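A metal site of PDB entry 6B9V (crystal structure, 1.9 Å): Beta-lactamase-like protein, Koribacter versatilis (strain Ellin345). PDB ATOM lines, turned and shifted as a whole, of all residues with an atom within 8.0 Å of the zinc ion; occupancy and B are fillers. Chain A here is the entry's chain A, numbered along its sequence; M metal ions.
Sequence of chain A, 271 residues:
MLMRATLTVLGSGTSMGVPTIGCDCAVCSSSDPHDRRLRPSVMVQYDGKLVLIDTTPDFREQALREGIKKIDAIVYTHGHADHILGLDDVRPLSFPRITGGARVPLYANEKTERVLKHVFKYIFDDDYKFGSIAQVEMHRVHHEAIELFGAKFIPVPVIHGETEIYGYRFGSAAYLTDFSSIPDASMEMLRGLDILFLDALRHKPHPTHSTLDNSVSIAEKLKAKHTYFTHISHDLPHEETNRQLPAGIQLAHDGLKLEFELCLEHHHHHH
The zinc ion is bound by ND1 of His 234, SG of Cys 28, SG of Cys 23 and SG of Cys 25.
Within 4 Å of the zinc ion: Cys 23, Cys 25, Cys 28 and His 234. The nearest printed residue that does not touch the zinc ion is Thr 20 (4.8 Å).
The side-chain sulfur (SG) of Cys 28 sits close to the backbone NH (N) of Thr 20, at 3.3 Å. The side-chain sulfur (SG) of Cys 25 lies close to the backbone NH (N) of Val 27. The backbone carbonyl oxygen (O) of Cys 25 is in hydrogen-bond range of the side-chain hydroxyl (OG) of Ser 29, 2.9 Å away.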
ATOM      1  N   GLY A  17      26.605 -13.939  18.412  1.00  0.00           N
ATOM      2  CA  GLY A  17      27.173 -13.047  17.418  1.00  0.00           C
ATOM      3  C   GLY A  17      27.423 -11.652  17.960  1.00  0.00           C
ATOM      4  O   GLY A  17      27.140 -11.388  19.126  1.00  0.00           O
ATOM      5  N   VAL A  18      27.983 -10.777  17.124  1.00  0.00           N
ATOM      6  CA  VAL A  18      28.038  -9.336  17.431  1.00  0.00           C
ATOM      7  C   VAL A  18      27.501  -8.606  16.203  1.00  0.00           C
ATOM      8  O   VAL A  18      27.986  -8.822  15.078  1.00  0.00           O
ATOM      9  CB  VAL A  18      29.475  -8.856  17.768  1.00  0.00           C
ATOM     10  CG1 VAL A  18      29.448  -7.435  18.367  1.00  0.00           C
ATOM     11  CG2 VAL A  18      30.136  -9.817  18.760  1.00  0.00           C
ATOM     12  N   PRO A  19      26.471  -7.764  16.380  1.00  0.00           N
ATOM     13  CA  PRO A  19      25.796  -7.361  17.623  1.00  0.00           C
ATOM     14  C   PRO A  19      24.932  -8.469  18.219  1.00  0.00           C
ATOM     15  O   PRO A  19      24.613  -9.439  17.556  1.00  0.00           O
ATOM     16  CB  PRO A  19      24.880  -6.208  17.179  1.00  0.00           C
ATOM     17  CG  PRO A  19      25.241  -5.916  15.774  1.00  0.00           C
ATOM     18  CD  PRO A  19      25.896  -7.105  15.198  1.00  0.00           C
ATOM     19  N   THR A  20      24.561  -8.274  19.481  1.00  0.00           N
ATOM     20  CA  THR A  20      23.552  -9.092  20.151  1.00  0.00           C
ATOM     21  C   THR A  20      22.189  -8.473  19.883  1.00  0.00           C
ATOM     22  O   THR A  20      22.017  -7.269  20.069  1.00  0.00           O
ATOM     23  CB  THR A  20      23.822  -9.147  21.682  1.00  0.00           C
ATOM     24  OG1 THR A  20      25.035  -9.856  21.935  1.00  0.00           O
ATOM     25  CG2 THR A  20      22.671  -9.827  22.417  1.00  0.00           C
ATOM     26  N   ILE A  21      21.219  -9.282  19.449  1.00  0.00           N
ATOM     27  CA  ILE A  21      19.865  -8.774  19.219  1.00  0.00           C
ATOM     28  C   ILE A  21      19.337  -8.007  20.429  1.00  0.00           C
ATOM     29  O   ILE A  21      19.431  -8.490  21.557  1.00  0.00           O
ATOM     30  CB  ILE A  21      18.865  -9.911  18.898  1.00  0.00           C
ATOM     31  CG1 ILE A  21      19.337 -10.731  17.706  1.00  0.00           C
ATOM     32  CG2 ILE A  21      17.497  -9.314  18.567  1.00  0.00           C
ATOM     33  CD1 ILE A  21      18.351 -11.822  17.311  1.00  0.00           C
ATOM     34  N   GLY A  22      18.819  -6.803  20.183  1.00  0.00           N
ATOM     35  CA  GLY A  22      18.160  -6.013  21.217  1.00  0.00           C
ATOM     36  C   GLY A  22      19.089  -5.103  22.003  1.00  0.00           C
ATOM     37  O   GLY A  22      18.615  -4.261  22.774  1.00  0.00           O
ATOM     38  N   CYS A  23      20.403  -5.270  21.821  1.00  0.00           N
ATOM     39  CA  CYS A  23      21.394  -4.549  22.607  1.00  0.00           C
ATOM     40  C   CYS A  23      21.813  -3.255  21.924  1.00  0.00           C
ATOM     41  O   CYS A  23      22.116  -3.245  20.731  1.00  0.00           O
ATOM     42  CB  CYS A  23      22.634  -5.422  22.864  1.00  0.00           C
ATOM     43  SG  CYS A  23      23.880  -4.656  23.941  1.00  0.00           S
ATOM     44  N   ASP A  24      21.862  -2.176  22.695  1.00  0.00           N
ATOM     45  CA  ASP A  24      22.237  -0.882  22.153  1.00  0.00           C
ATOM     46  C   ASP A  24      23.576  -0.372  22.690  1.00  0.00           C
ATOM     47  O   ASP A  24      23.801   0.836  22.678  1.00  0.00           O
ATOM     48  CB  ASP A  24      21.147   0.153  22.432  1.00  0.00           C
ATOM     49  CG  ASP A  24      19.840  -0.179  21.739  1.00  0.00           C
ATOM     50  OD1 ASP A  24      19.878  -0.647  20.585  1.00  0.00           O
ATOM     51  OD2 ASP A  24      18.779   0.033  22.363  1.00  0.00           O
ATOM     52  N   CYS A  25      24.453  -1.266  23.131  1.00  0.00           N
ATOM     53  CA  CYS A  25      25.731  -0.851  23.721  1.00  0.00           C
ATOM     54  C   CYS A  25      26.664  -0.298  22.632  1.00  0.00           C
ATOM     55  O   CYS A  25      26.371  -0.401  21.434  1.00  0.00           O
ATOM     56  CB  CYS A  25      26.408  -2.017  24.451  1.00  0.00           C
ATOM     57  SG  CYS A  25      27.302  -3.192  23.380  1.00  0.00           S
ATOM     58  N   ALA A  26      27.791   0.285  23.054  1.00  0.00           N
ATOM     59  CA  ALA A  26      28.711   0.918  22.108  1.00  0.00           C
ATOM     60  C   ALA A  26      29.158  -0.029  21.001  1.00  0.00           C
ATOM     61  O   ALA A  26      29.121   0.349  19.825  1.00  0.00           O
ATOM     62  CB  ALA A  26      29.938   1.475  22.851  1.00  0.00           C
ATOM     63  N   VAL A  27      29.556  -1.239  21.362  1.00  0.00           N
ATOM     64  CA  VAL A  27      30.065  -2.181  20.357  1.00  0.00           C
ATOM     65  C   VAL A  27      28.941  -2.667  19.417  1.00  0.00           C
ATOM     66  O   VAL A  27      29.121  -2.750  18.194  1.00  0.00           O
ATOM     67  CB  VAL A  27      30.797  -3.376  21.028  1.00  0.00           C
ATOM     68  CG1 VAL A  27      31.221  -4.442  20.002  1.00  0.00           C
ATOM     69  CG2 VAL A  27      32.025  -2.857  21.789  1.00  0.00           C
ATOM     70  N   CYS A  28      27.767  -2.946  19.974  1.00  0.00           N
ATOM     71  CA  CYS A  28      26.648  -3.388  19.127  1.00  0.00           C
ATOM     72  C   CYS A  28      26.158  -2.263  18.218  1.00  0.00           C
ATOM     73  O   CYS A  28      25.522  -2.531  17.196  1.00  0.00           O
ATOM     74  CB  CYS A  28      25.499  -3.942  19.988  1.00  0.00           C
ATOM     75  SG  CYS A  28      25.901  -5.568  20.738  1.00  0.00           S
ATOM     76  N   SER A  29      26.470  -1.027  18.569  1.00  0.00           N
ATOM     77  CA  SER A  29      26.060   0.147  17.803  1.00  0.00           C
ATOM     78  C   SER A  29      27.161   0.586  16.862  1.00  0.00           C
ATOM     79  O   SER A  29      26.995   1.543  16.127  1.00  0.00           O
ATOM     80  CB  SER A  29      25.684   1.319  18.737  1.00  0.00           C
ATOM     81  OG  SER A  29      24.634   0.957  19.600  1.00  0.00           O
ATOM     82  N   SER A 233      32.917 -11.558  21.983  1.00  0.00           N
ATOM     83  CA  SER A 233      31.605 -10.994  22.358  1.00  0.00           C
ATOM     84  C   SER A 233      31.578  -9.472  22.242  1.00  0.00           C
ATOM     85  O   SER A 233      32.604  -8.835  21.968  1.00  0.00           O
ATOM     86  CB  SER A 233      31.248 -11.400  23.794  1.00  0.00           C
ATOM     87  OG  SER A 233      31.966 -10.587  24.728  1.00  0.00           O
ATOM     88  N   HIS A 234      30.407  -8.855  22.470  1.00  0.00           N
ATOM     89  CA  HIS A 234      30.320  -7.395  22.399  1.00  0.00           C
ATOM     90  C   HIS A 234      31.084  -6.677  23.510  1.00  0.00           C
ATOM     91  O   HIS A 234      31.163  -5.445  23.551  1.00  0.00           O
ATOM     92  CB  HIS A 234      28.839  -6.937  22.342  1.00  0.00           C
ATOM     93  CG  HIS A 234      28.008  -7.301  23.548  1.00  0.00           C
ATOM     94  ND1 HIS A 234      26.843  -6.664  23.896  1.00  0.00           N
ATOM     95  CD2 HIS A 234      28.247  -8.201  24.533  1.00  0.00           C
ATOM     96  CE1 HIS A 234      26.366  -7.181  25.013  1.00  0.00           C
ATOM     97  NE2 HIS A 234      27.202  -8.121  25.416  1.00  0.00           N
ATOM     98  N   ASP A 235      31.678  -7.448  24.412  1.00  0.00           N
ATOM     99  CA  ASP A 235      32.510  -6.876  25.465  1.00  0.00           C
ATOM    100  C   ASP A 235      33.810  -6.289  24.919  1.00  0.00           C
ATOM    101  O   ASP A 235      34.442  -5.486  25.601  1.00  0.00           O
ATOM    102  CB  ASP A 235      32.836  -7.934  26.524  1.00  0.00           C
ATOM    103  CG  ASP A 235      33.235  -7.337  27.849  1.00  0.00           C
ATOM    104  OD1 ASP A 235      32.472  -6.493  28.364  1.00  0.00           O
ATOM    105  OD2 ASP A 235      34.321  -7.688  28.375  1.00  0.00           O
HETATM  106 ZN    ZN M   1      25.953  -5.057  22.982  1.00  0.00          ZN
